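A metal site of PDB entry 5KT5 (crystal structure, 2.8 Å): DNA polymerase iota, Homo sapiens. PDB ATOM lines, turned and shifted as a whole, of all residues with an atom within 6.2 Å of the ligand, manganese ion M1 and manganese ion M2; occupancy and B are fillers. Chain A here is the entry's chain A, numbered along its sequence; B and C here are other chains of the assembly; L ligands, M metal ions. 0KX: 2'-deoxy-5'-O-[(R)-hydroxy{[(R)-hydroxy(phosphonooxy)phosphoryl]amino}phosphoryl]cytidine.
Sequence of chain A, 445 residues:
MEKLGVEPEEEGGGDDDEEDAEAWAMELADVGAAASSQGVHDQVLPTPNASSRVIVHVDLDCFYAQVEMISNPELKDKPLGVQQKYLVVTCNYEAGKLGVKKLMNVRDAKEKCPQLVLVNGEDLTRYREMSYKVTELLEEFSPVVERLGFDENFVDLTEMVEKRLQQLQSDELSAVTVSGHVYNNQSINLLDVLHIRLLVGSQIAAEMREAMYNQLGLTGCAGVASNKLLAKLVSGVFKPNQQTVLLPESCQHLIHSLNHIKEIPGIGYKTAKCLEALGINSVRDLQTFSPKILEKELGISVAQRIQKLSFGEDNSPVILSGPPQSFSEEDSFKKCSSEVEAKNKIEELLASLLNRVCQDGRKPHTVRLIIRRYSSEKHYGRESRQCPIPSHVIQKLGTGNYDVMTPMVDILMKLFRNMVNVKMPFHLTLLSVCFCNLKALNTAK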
ATOM      1  N   ASP A  59     -18.708 -13.731 -22.055  1.00  0.00           N
ATOM      2  CA  ASP A  59     -20.141 -13.888 -22.251  1.00  0.00           C
ATOM      3  C   ASP A  59     -20.860 -12.881 -21.352  1.00  0.00           C
ATOM      4  O   ASP A  59     -20.611 -12.847 -20.144  1.00  0.00           O
ATOM      5  CB  ASP A  59     -20.581 -15.317 -21.908  1.00  0.00           C
ATOM      6  CG  ASP A  59     -22.072 -15.562 -22.128  1.00  0.00           C
ATOM      7  OD1 ASP A  59     -22.415 -16.546 -22.809  1.00  0.00           O
ATOM      8  OD2 ASP A  59     -22.907 -14.798 -21.610  1.00  0.00           O
ATOM      9  N   LEU A  60     -21.748 -12.092 -21.923  1.00  0.00           N
ATOM     10  CA  LEU A  60     -22.400 -11.019 -21.174  1.00  0.00           C
ATOM     11  C   LEU A  60     -23.520 -11.576 -20.301  1.00  0.00           C
ATOM     12  O   LEU A  60     -24.254 -12.472 -20.701  1.00  0.00           O
ATOM     13  CB  LEU A  60     -22.955  -9.972 -22.128  1.00  0.00           C
ATOM     14  CG  LEU A  60     -21.871  -9.333 -22.999  1.00  0.00           C
ATOM     15  CD1 LEU A  60     -22.426  -8.201 -23.839  1.00  0.00           C
ATOM     16  CD2 LEU A  60     -20.754  -8.836 -22.107  1.00  0.00           C
ATOM     17  N   ASP A  61     -23.629 -11.019 -19.091  1.00  0.00           N
ATOM     18  CA  ASP A  61     -24.710 -11.386 -18.181  1.00  0.00           C
ATOM     19  C   ASP A  61     -26.046 -10.885 -18.711  1.00  0.00           C
ATOM     20  O   ASP A  61     -26.183  -9.697 -19.013  1.00  0.00           O
ATOM     21  CB  ASP A  61     -24.445 -10.794 -16.800  1.00  0.00           C
ATOM     22  CG  ASP A  61     -23.096 -11.214 -16.214  1.00  0.00           C
ATOM     23  OD1 ASP A  61     -22.787 -12.429 -16.205  1.00  0.00           O
ATOM     24  OD2 ASP A  61     -22.348 -10.325 -15.766  1.00  0.00           O
ATOM     25  N   CYS A  62     -27.023 -11.802 -18.793  1.00  0.00           N
ATOM     26  CA  CYS A  62     -28.377 -11.548 -19.282  1.00  0.00           C
ATOM     27  C   CYS A  62     -28.434 -10.387 -20.263  1.00  0.00           C
ATOM     28  O   CYS A  62     -28.971  -9.320 -19.953  1.00  0.00           O
ATOM     29  CB  CYS A  62     -29.339 -11.293 -18.107  1.00  0.00           C
ATOM     30  SG  CYS A  62     -28.746 -10.097 -16.880  1.00  0.00           S
ATOM     31  N   PHE A  63     -27.874 -10.597 -21.455  1.00  0.00           N
ATOM     32  CA  PHE A  63     -27.458  -9.491 -22.304  1.00  0.00           C
ATOM     33  C   PHE A  63     -28.605  -8.513 -22.585  1.00  0.00           C
ATOM     34  O   PHE A  63     -28.571  -7.343 -22.187  1.00  0.00           O
ATOM     35  CB  PHE A  63     -26.856 -10.047 -23.591  1.00  0.00           C
ATOM     36  CG  PHE A  63     -26.426  -8.979 -24.570  1.00  0.00           C
ATOM     37  CD1 PHE A  63     -25.793  -7.821 -24.148  1.00  0.00           C
ATOM     38  CD2 PHE A  63     -26.664  -9.148 -25.932  1.00  0.00           C
ATOM     39  CE1 PHE A  63     -25.407  -6.852 -25.054  1.00  0.00           C
ATOM     40  CE2 PHE A  63     -26.287  -8.183 -26.834  1.00  0.00           C
ATOM     41  CZ  PHE A  63     -25.654  -7.033 -26.397  1.00  0.00           C
ATOM     42  N   TYR A  64     -29.639  -8.999 -23.282  1.00  0.00           N
ATOM     43  CA  TYR A  64     -30.780  -8.154 -23.615  1.00  0.00           C
ATOM     44  C   TYR A  64     -31.344  -7.453 -22.382  1.00  0.00           C
ATOM     45  O   TYR A  64     -31.603  -6.240 -22.395  1.00  0.00           O
ATOM     46  CB  TYR A  64     -31.879  -8.989 -24.289  1.00  0.00           C
ATOM     47  CG  TYR A  64     -31.528  -9.543 -25.654  1.00  0.00           C
ATOM     48  CD1 TYR A  64     -30.281  -9.326 -26.240  1.00  0.00           C
ATOM     49  CD2 TYR A  64     -32.459 -10.267 -26.388  1.00  0.00           C
ATOM     50  CE1 TYR A  64     -29.971  -9.830 -27.490  1.00  0.00           C
ATOM     51  CE2 TYR A  64     -32.157 -10.776 -27.635  1.00  0.00           C
ATOM     52  CZ  TYR A  64     -30.917 -10.560 -28.184  1.00  0.00           C
ATOM     53  OH  TYR A  64     -30.629 -11.067 -29.430  1.00  0.00           O
ATOM     54  N   ALA A  65     -31.535  -8.211 -21.294  1.00  0.00           N
ATOM     55  CA  ALA A  65     -32.081  -7.618 -20.082  1.00  0.00           C
ATOM     56  C   ALA A  65     -31.146  -6.552 -19.512  1.00  0.00           C
ATOM     57  O   ALA A  65     -31.597  -5.551 -18.941  1.00  0.00           O
ATOM     58  CB  ALA A  65     -32.347  -8.695 -19.034  1.00  0.00           C
ATOM     59  N   GLN A  84     -39.974 -12.041 -26.766  1.00  0.00           N
ATOM     60  CA  GLN A  84     -40.127 -12.033 -28.228  1.00  0.00           C
ATOM     61  C   GLN A  84     -41.240 -13.019 -28.558  1.00  0.00           C
ATOM     62  O   GLN A  84     -41.071 -14.225 -28.376  1.00  0.00           O
ATOM     63  CB  GLN A  84     -38.830 -12.418 -28.934  1.00  0.00           C
ATOM     64  CG  GLN A  84     -37.696 -11.423 -28.763  1.00  0.00           C
ATOM     65  CD  GLN A  84     -36.390 -11.934 -29.316  1.00  0.00           C
ATOM     66  OE1 GLN A  84     -36.131 -13.145 -29.327  1.00  0.00           O
ATOM     67  NE2 GLN A  84     -35.550 -11.024 -29.783  1.00  0.00           N
ATOM     68  N   VAL A  89     -37.032 -14.549 -23.690  1.00  0.00           N
ATOM     69  CA  VAL A  89     -35.753 -14.962 -24.251  1.00  0.00           C
ATOM     70  C   VAL A  89     -34.626 -14.853 -23.228  1.00  0.00           C
ATOM     71  O   VAL A  89     -33.611 -15.559 -23.334  1.00  0.00           O
ATOM     72  CB  VAL A  89     -35.449 -14.159 -25.527  1.00  0.00           C
ATOM     73  CG1 VAL A  89     -34.650 -12.897 -25.207  1.00  0.00           C
ATOM     74  CG2 VAL A  89     -34.715 -15.019 -26.523  1.00  0.00           C
ATOM     75  N   THR A  90     -34.768 -13.961 -22.244  1.00  0.00           N
ATOM     76  CA  THR A  90     -33.821 -13.865 -21.136  1.00  0.00           C
ATOM     77  C   THR A  90     -34.438 -12.995 -20.065  1.00  0.00           C
ATOM     78  O   THR A  90     -35.491 -12.369 -20.256  1.00  0.00           O
ATOM     79  CB  THR A  90     -32.462 -13.284 -21.573  1.00  0.00           C
ATOM     80  OG1 THR A  90     -31.550 -13.358 -20.467  1.00  0.00           O
ATOM     81  CG2 THR A  90     -32.615 -11.837 -22.001  1.00  0.00           C
ATOM     82  N   CYS A  91     -33.774 -12.961 -18.914  1.00  0.00           N
ATOM     83  CA  CYS A  91     -34.310 -12.259 -17.754  1.00  0.00           C
ATOM     84  C   CYS A  91     -33.161 -11.832 -16.860  1.00  0.00           C
ATOM     85  O   CYS A  91     -32.077 -12.426 -16.888  1.00  0.00           O
ATOM     86  CB  CYS A  91     -35.312 -13.131 -16.989  1.00  0.00           C
ATOM     87  SG  CYS A  91     -34.613 -14.600 -16.201  1.00  0.00           S
ATOM     88  N   LYS A 102     -34.299 -18.753 -18.900  1.00  0.00           N
ATOM     89  CA  LYS A 102     -34.142 -18.305 -20.280  1.00  0.00           C
ATOM     90  C   LYS A 102     -34.900 -19.222 -21.222  1.00  0.00           C
ATOM     91  O   LYS A 102     -34.928 -20.447 -21.054  1.00  0.00           O
ATOM     92  CB  LYS A 102     -32.656 -18.264 -20.638  1.00  0.00           C
ATOM     93  CG  LYS A 102     -31.846 -17.283 -19.797  1.00  0.00           C
ATOM     94  CD  LYS A 102     -30.355 -17.392 -20.045  1.00  0.00           C
ATOM     95  CE  LYS A 102     -29.754 -18.623 -19.373  1.00  0.00           C
ATOM     96  NZ  LYS A 102     -28.255 -18.617 -19.399  1.00  0.00           N
ATOM     97  N   LEU A 103     -35.529 -18.615 -22.237  1.00  0.00           N
ATOM     98  CA  LEU A 103     -36.298 -19.336 -23.245  1.00  0.00           C
ATOM     99  C   LEU A 103     -37.507 -20.061 -22.649  1.00  0.00           C
ATOM    100  O   LEU A 103     -37.930 -21.113 -23.131  1.00  0.00           O
ATOM    101  CB  LEU A 103     -35.409 -20.323 -24.023  1.00  0.00           C
ATOM    102  CG  LEU A 103     -34.144 -19.690 -24.619  1.00  0.00           C
ATOM    103  CD1 LEU A 103     -33.208 -20.751 -25.174  1.00  0.00           C
ATOM    104  CD2 LEU A 103     -34.509 -18.694 -25.692  1.00  0.00           C
ATOM    105  N   LEU A 124     -33.705  -5.992 -32.448  1.00  0.00           N
ATOM    106  CA  LEU A 124     -32.358  -6.246 -31.946  1.00  0.00           C
ATOM    107  C   LEU A 124     -31.390  -5.092 -32.221  1.00  0.00           C
ATOM    108  O   LEU A 124     -30.175  -5.297 -32.105  1.00  0.00           O
ATOM    109  CB  LEU A 124     -31.803  -7.524 -32.577  1.00  0.00           C
ATOM    110  CG  LEU A 124     -32.697  -8.766 -32.666  1.00  0.00           C
ATOM    111  CD1 LEU A 124     -31.893  -9.934 -33.213  1.00  0.00           C
ATOM    112  CD2 LEU A 124     -33.311  -9.112 -31.319  1.00  0.00           C
ATOM    113  N   LEU A 148     -19.042 -14.945 -31.207  1.00  0.00           N
ATOM    114  CA  LEU A 148     -20.039 -16.000 -31.137  1.00  0.00           C
ATOM    115  C   LEU A 148     -21.322 -15.387 -30.588  1.00  0.00           C
ATOM    116  O   LEU A 148     -21.332 -14.882 -29.452  1.00  0.00           O
ATOM    117  CB  LEU A 148     -19.579 -17.183 -30.268  1.00  0.00           C
ATOM    118  CG  LEU A 148     -20.414 -18.452 -30.429  1.00  0.00           C
ATOM    119  CD1 LEU A 148     -20.523 -18.828 -31.895  1.00  0.00           C
ATOM    120  CD2 LEU A 148     -19.835 -19.609 -29.624  1.00  0.00           C
ATOM    121  N   PHE A 150     -24.418 -12.631 -30.297  1.00  0.00           N
ATOM    122  CA  PHE A 150     -24.301 -11.204 -30.034  1.00  0.00           C
ATOM    123  C   PHE A 150     -23.506 -10.908 -28.770  1.00  0.00           C
ATOM    124  O   PHE A 150     -23.044  -9.771 -28.609  1.00  0.00           O
ATOM    125  CB  PHE A 150     -25.688 -10.579 -29.910  1.00  0.00           C
ATOM    126  CG  PHE A 150     -26.341 -10.271 -31.237  1.00  0.00           C
ATOM    127  CD1 PHE A 150     -27.500  -9.516 -31.295  1.00  0.00           C
ATOM    128  CD2 PHE A 150     -25.801 -10.731 -32.422  1.00  0.00           C
ATOM    129  CE1 PHE A 150     -28.104  -9.220 -32.504  1.00  0.00           C
ATOM    130  CE2 PHE A 150     -26.385 -10.449 -33.636  1.00  0.00           C
ATOM    131  CZ  PHE A 150     -27.537  -9.696 -33.682  1.00  0.00           C
ATOM    132  N   ASP A 151     -23.318 -11.877 -27.880  1.00  0.00           N
ATOM    133  CA  ASP A 151     -22.809 -11.580 -26.552  1.00  0.00           C
ATOM    134  C   ASP A 151     -21.576 -12.387 -26.158  1.00  0.00           C
ATOM    135  O   ASP A 151     -21.191 -12.356 -24.988  1.00  0.00           O
ATOM    136  CB  ASP A 151     -23.910 -11.772 -25.509  1.00  0.00           C
ATOM    137  CG  ASP A 151     -23.972 -13.188 -24.959  1.00  0.00           C
ATOM    138  OD1 ASP A 151     -23.876 -14.153 -25.757  1.00  0.00           O
ATOM    139  OD2 ASP A 151     -24.097 -13.342 -23.719  1.00  0.00           O
ATOM    140  N   GLU A 152     -20.940 -13.114 -27.083  1.00  0.00           N
ATOM    141  CA  GLU A 152     -19.750 -13.877 -26.723  1.00  0.00           C
ATOM    142  C   GLU A 152     -18.594 -13.539 -27.647  1.00  0.00           C
ATOM    143  O   GLU A 152     -18.780 -13.319 -28.846  1.00  0.00           O
ATOM    144  CB  GLU A 152     -20.041 -15.378 -26.726  1.00  0.00           C
ATOM    145  CG  GLU A 152     -20.990 -15.784 -25.610  1.00  0.00           C
ATOM    146  CD  GLU A 152     -21.409 -17.228 -25.703  1.00  0.00           C
ATOM    147  OE1 GLU A 152     -20.604 -18.050 -26.172  1.00  0.00           O
ATOM    148  OE2 GLU A 152     -22.545 -17.542 -25.305  1.00  0.00           O
ATOM    149  N   LYS A 239     -21.078 -17.448 -12.062  1.00  0.00           N
ATOM    150  CA  LYS A 239     -21.952 -16.449 -12.652  1.00  0.00           C
ATOM    151  C   LYS A 239     -22.803 -15.775 -11.581  1.00  0.00           C
ATOM    152  O   LYS A 239     -23.147 -16.412 -10.582  1.00  0.00           O
ATOM    153  CB  LYS A 239     -22.853 -17.090 -13.727  1.00  0.00           C
ATOM    154  CG  LYS A 239     -22.136 -17.429 -15.025  1.00  0.00           C
ATOM    155  CD  LYS A 239     -22.965 -18.350 -15.910  1.00  0.00           C
ATOM    156  CE  LYS A 239     -24.407 -17.870 -16.044  1.00  0.00           C
ATOM    157  NZ  LYS A 239     -25.209 -18.755 -16.931  1.00  0.00           N
ATOM    158  N   PRO A 240     -23.138 -14.493 -11.777  1.00  0.00           N
ATOM    159  CA  PRO A 240     -22.712 -13.653 -12.903  1.00  0.00           C
ATOM    160  C   PRO A 240     -21.523 -12.769 -12.569  1.00  0.00           C
ATOM    161  O   PRO A 240     -21.095 -12.737 -11.414  1.00  0.00           O
ATOM    162  CB  PRO A 240     -23.950 -12.797 -13.161  1.00  0.00           C
ATOM    163  CG  PRO A 240     -24.490 -12.565 -11.786  1.00  0.00           C
ATOM    164  CD  PRO A 240     -24.186 -13.823 -10.973  1.00  0.00           C
ATOM    165  P    DC B   7     -23.882 -22.127 -27.646  1.00  0.00           P
ATOM    166  OP1  DC B   7     -22.967 -22.271 -26.489  1.00  0.00           O
ATOM    167  OP2  DC B   7     -24.978 -23.103 -27.844  1.00  0.00           O
ATOM    168  O5'  DC B   7     -24.508 -20.662 -27.626  1.00  0.00           O
ATOM    169  C5'  DC B   7     -23.639 -19.529 -27.600  1.00  0.00           C
ATOM    170  C4'  DC B   7     -24.404 -18.240 -27.870  1.00  0.00           C
ATOM    171  O4'  DC B   7     -24.933 -18.263 -29.204  1.00  0.00           O
ATOM    172  C3'  DC B   7     -25.623 -17.999 -26.996  1.00  0.00           C
ATOM    173  O3'  DC B   7     -25.225 -17.466 -25.734  1.00  0.00           O
ATOM    174  C2'  DC B   7     -26.381 -16.976 -27.821  1.00  0.00           C
ATOM    175  C1'  DC B   7     -26.087 -17.432 -29.259  1.00  0.00           C
ATOM    176  N1   DC B   7     -27.196 -18.201 -29.866  1.00  0.00           N
ATOM    177  C2   DC B   7     -28.301 -17.518 -30.364  1.00  0.00           C
ATOM    178  O2   DC B   7     -28.305 -16.290 -30.298  1.00  0.00           O
ATOM    179  N3   DC B   7     -29.328 -18.230 -30.909  1.00  0.00           N
ATOM    180  C4   DC B   7     -29.261 -19.559 -30.946  1.00  0.00           C
ATOM    181  N4   DC B   7     -30.286 -20.212 -31.490  1.00  0.00           N
ATOM    182  C5   DC B   7     -28.141 -20.281 -30.439  1.00  0.00           C
ATOM    183  C6   DC B   7     -27.135 -19.565 -29.907  1.00  0.00           C
ATOM    184  P    DG C   3     -42.521 -18.468 -31.622  1.00  0.00           P
ATOM    185  OP1  DG C   3     -43.972 -18.221 -31.702  1.00  0.00           O
ATOM    186  OP2  DG C   3     -41.860 -19.296 -32.653  1.00  0.00           O
ATOM    187  O5'  DG C   3     -41.732 -17.081 -31.595  1.00  0.00           O
ATOM    188  C5'  DG C   3     -40.440 -17.023 -30.990  1.00  0.00           C
ATOM    189  C4'  DG C   3     -39.859 -15.629 -31.048  1.00  0.00           C
ATOM    190  O4'  DG C   3     -38.605 -15.599 -30.319  1.00  0.00           O
ATOM    191  C3'  DG C   3     -39.519 -15.116 -32.439  1.00  0.00           C
ATOM    192  O3'  DG C   3     -39.543 -13.697 -32.435  1.00  0.00           O
ATOM    193  C2'  DG C   3     -38.105 -15.652 -32.629  1.00  0.00           C
ATOM    194  C1'  DG C   3     -37.527 -15.467 -31.219  1.00  0.00           C
ATOM    195  N9   DG C   3     -36.485 -16.435 -30.852  1.00  0.00           N
ATOM    196  C8   DG C   3     -35.305 -16.150 -30.216  1.00  0.00           C
ATOM    197  N7   DG C   3     -34.573 -17.207 -29.984  1.00  0.00           N
ATOM    198  C5   DG C   3     -35.320 -18.262 -30.487  1.00  0.00           C
ATOM    199  C6   DG C   3     -35.040 -19.645 -30.516  1.00  0.00           C
ATOM    200  O6   DG C   3     -34.036 -20.241 -30.094  1.00  0.00           O
ATOM    201  N1   DG C   3     -36.071 -20.375 -31.120  1.00  0.00           N
ATOM    202  C2   DG C   3     -37.225 -19.818 -31.620  1.00  0.00           C
ATOM    203  N2   DG C   3     -38.097 -20.678 -32.165  1.00  0.00           N
ATOM    204  N3   DG C   3     -37.505 -18.522 -31.598  1.00  0.00           N
ATOM    205  C4   DG C   3     -36.513 -17.808 -31.016  1.00  0.00           C
ATOM    206  P    DG C   4     -39.708 -12.862 -33.807  1.00  0.00           P
ATOM    207  OP1  DG C   4     -40.629 -11.733 -33.538  1.00  0.00           O
ATOM    208  OP2  DG C   4     -40.007 -13.813 -34.895  1.00  0.00           O
ATOM    209  O5'  DG C   4     -38.245 -12.273 -34.063  1.00  0.00           O
ATOM    210  C5'  DG C   4     -37.594 -11.533 -33.041  1.00  0.00           C
ATOM    211  C4'  DG C   4     -36.102 -11.458 -33.315  1.00  0.00           C
ATOM    212  O4'  DG C   4     -35.464 -12.670 -32.809  1.00  0.00           O
ATOM    213  C3'  DG C   4     -35.727 -11.379 -34.795  1.00  0.00           C
ATOM    214  O3'  DG C   4     -34.657 -10.443 -34.977  1.00  0.00           O
ATOM    215  C2'  DG C   4     -35.284 -12.801 -35.097  1.00  0.00           C
ATOM    216  C1'  DG C   4     -34.603 -13.153 -33.794  1.00  0.00           C
ATOM    217  N9   DG C   4     -34.357 -14.587 -33.640  1.00  0.00           N
ATOM    218  C8   DG C   4     -35.136 -15.622 -34.104  1.00  0.00           C
ATOM    219  N7   DG C   4     -34.639 -16.802 -33.834  1.00  0.00           N
ATOM    220  C5   DG C   4     -33.467 -16.526 -33.145  1.00  0.00           C
ATOM    221  C6   DG C   4     -32.502 -17.402 -32.602  1.00  0.00           C
ATOM    222  O6   DG C   4     -32.498 -18.641 -32.604  1.00  0.00           O
ATOM    223  N1   DG C   4     -31.461 -16.703 -31.993  1.00  0.00           N
ATOM    224  C2   DG C   4     -31.364 -15.333 -31.927  1.00  0.00           C
ATOM    225  N2   DG C   4     -30.291 -14.829 -31.314  1.00  0.00           N
ATOM    226  N3   DG C   4     -32.264 -14.501 -32.441  1.00  0.00           N
ATOM    227  C4   DG C   4     -33.278 -15.169 -33.035  1.00  0.00           C
HETATM  228  PG  0KX L   1     -26.366 -15.309 -19.164  1.00  0.00           P
HETATM  229  O1G 0KX L   1     -25.281 -15.173 -20.208  1.00  0.00           O
HETATM  230  O2G 0KX L   1     -26.815 -16.739 -18.948  1.00  0.00           O
HETATM  231  O3G 0KX L   1     -26.102 -14.538 -17.898  1.00  0.00           O
HETATM  232  PB  0KX L   1     -27.859 -14.417 -21.390  1.00  0.00           P
HETATM  233  O1B 0KX L   1     -29.184 -13.706 -21.566  1.00  0.00           O
HETATM  234  O2B 0KX L   1     -26.634 -13.728 -21.945  1.00  0.00           O
HETATM  235  O3B 0KX L   1     -27.652 -14.584 -19.806  1.00  0.00           O
HETATM  236  PA  0KX L   1     -27.130 -16.223 -23.625  1.00  0.00           P
HETATM  237  O1A 0KX L   1     -27.343 -17.656 -24.049  1.00  0.00           O
HETATM  238  O2A 0KX L   1     -25.703 -15.754 -23.436  1.00  0.00           O
HETATM  239  N3A 0KX L   1     -28.018 -16.021 -22.114  1.00  0.00           N
HETATM  240  O5' 0KX L   1     -27.753 -15.306 -24.787  1.00  0.00           O
HETATM  241  C5' 0KX L   1     -27.325 -13.956 -24.988  1.00  0.00           C
HETATM  242  C4' 0KX L   1     -28.512 -13.205 -25.575  1.00  0.00           C
HETATM  243  O4' 0KX L   1     -28.855 -13.752 -26.846  1.00  0.00           O
HETATM  244  C3' 0KX L   1     -29.739 -13.362 -24.701  1.00  0.00           C
HETATM  245  O3' 0KX L   1     -29.922 -12.237 -23.824  1.00  0.00           O
HETATM  246  C2' 0KX L   1     -30.902 -13.475 -25.671  1.00  0.00           C
HETATM  247  C1' 0KX L   1     -30.276 -13.842 -27.012  1.00  0.00           C
HETATM  248  N1  0KX L   1     -30.671 -15.212 -27.336  1.00  0.00           N
HETATM  249  C2  0KX L   1     -31.772 -15.482 -28.163  1.00  0.00           C
HETATM  250  N3  0KX L   1     -32.122 -16.758 -28.430  1.00  0.00           N
HETATM  251  C4  0KX L   1     -31.412 -17.789 -27.909  1.00  0.00           C
HETATM  252  C5  0KX L   1     -30.320 -17.533 -27.095  1.00  0.00           C
HETATM  253  C6  0KX L   1     -29.964 -16.218 -26.817  1.00  0.00           C
HETATM  254  O2  0KX L   1     -32.439 -14.537 -28.651  1.00  0.00           O
HETATM  255  N4  0KX L   1     -31.763 -19.070 -28.185  1.00  0.00           N
HETATM  256 MN    MN M   1     -24.781 -14.182 -21.951  1.00  0.00          MN
HETATM  257 MN    MN M   2     -24.134 -16.168 -24.328  1.00  0.00          MN
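The side-chain amino group (NZ) of Lys 102 lies within salt-bridge range of an oxygen (O2G) of the ligand. An oxygen (O1B) of the ligand sits at hydrogen-bond distance from the side-chain hydroxyl of Thr 90 (2.6 Å). O6 of DG 3 of chain C is in hydrogen-bond range of N4 of the ligand (3.2 Å). An oxygen (O3G) of the ligand is in hydrogen-bond range of the backbone NH of Cys 62 (3.0 Å). The side-chain amino group (NZ) of Lys 239 lies within salt-bridge range of an oxygen (O2G) of the ligand (3.3 Å). An oxygen (O3') of the ligand lies within hydrogen-bond range of the backbone NH of Tyr 64. The backbone NH (N) of Phe 63 sits at hydrogen-bond distance from an oxygen (O1B) of the ligand, 3.4 Å away.
O2 of DC 7 of chain B sits close to N2 of DG 4 of chain C (2.7 Å). O4' of DG 4 of chain C lies within hydrogen-bond range of NE2 of Gln 84 (3.4 Å).
N2 of DG 4 of chain C sits close to an oxygen (O2) of the ligand, at 3.4 Å. Asp 61 touches the ligand (CA to O3G, 3.5 Å). CG2 of Val 89 touches O2 of the ligand, at 3.2 Å. CD2 of Leu 103 touches N4 of the ligand, 3.7 Å away. Hydrophobic or aromatic side chains that line the ligand: Phe 63, Tyr 64, Val 89 and Leu 103. Of the 23 residues printed, 15 come within 4 Å of the ligand.
The nearest printed residue that does not touch manganese ion M1 is Asp 61 (4.4 Å).
Within 4 Å of manganese ion M2: Asp 59, Asp 151, Glu 152 and DC 7 of chain B.
Manganese ion M1 is bound by an oxygen (O2B) of the ligand, the side-chain carboxylate of Asp 59, an oxygen (O1G) of the ligand, the side-chain carboxylate of Asp 151, the backbone carbonyl oxygen of Leu 60 and an oxygen (O2A) of the ligand. Manganese ion M1 has six donor atoms within binding distance.
Manganese ion M2 is bound by O2A of the ligand (1.9 Å), O3' of DC 7 of chain B (2.2 Å), OE2 of Glu 152 (2.3 Å), OD1 of Asp 59 (2.3 Å) and OD1 of Asp 151 (2.5 Å). Manganese ion M2 has five donor atoms within binding distance. Slightly farther from manganese ion M2 lies the side-chain carboxylate (OD2) of Asp 151 (2.9 Å).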
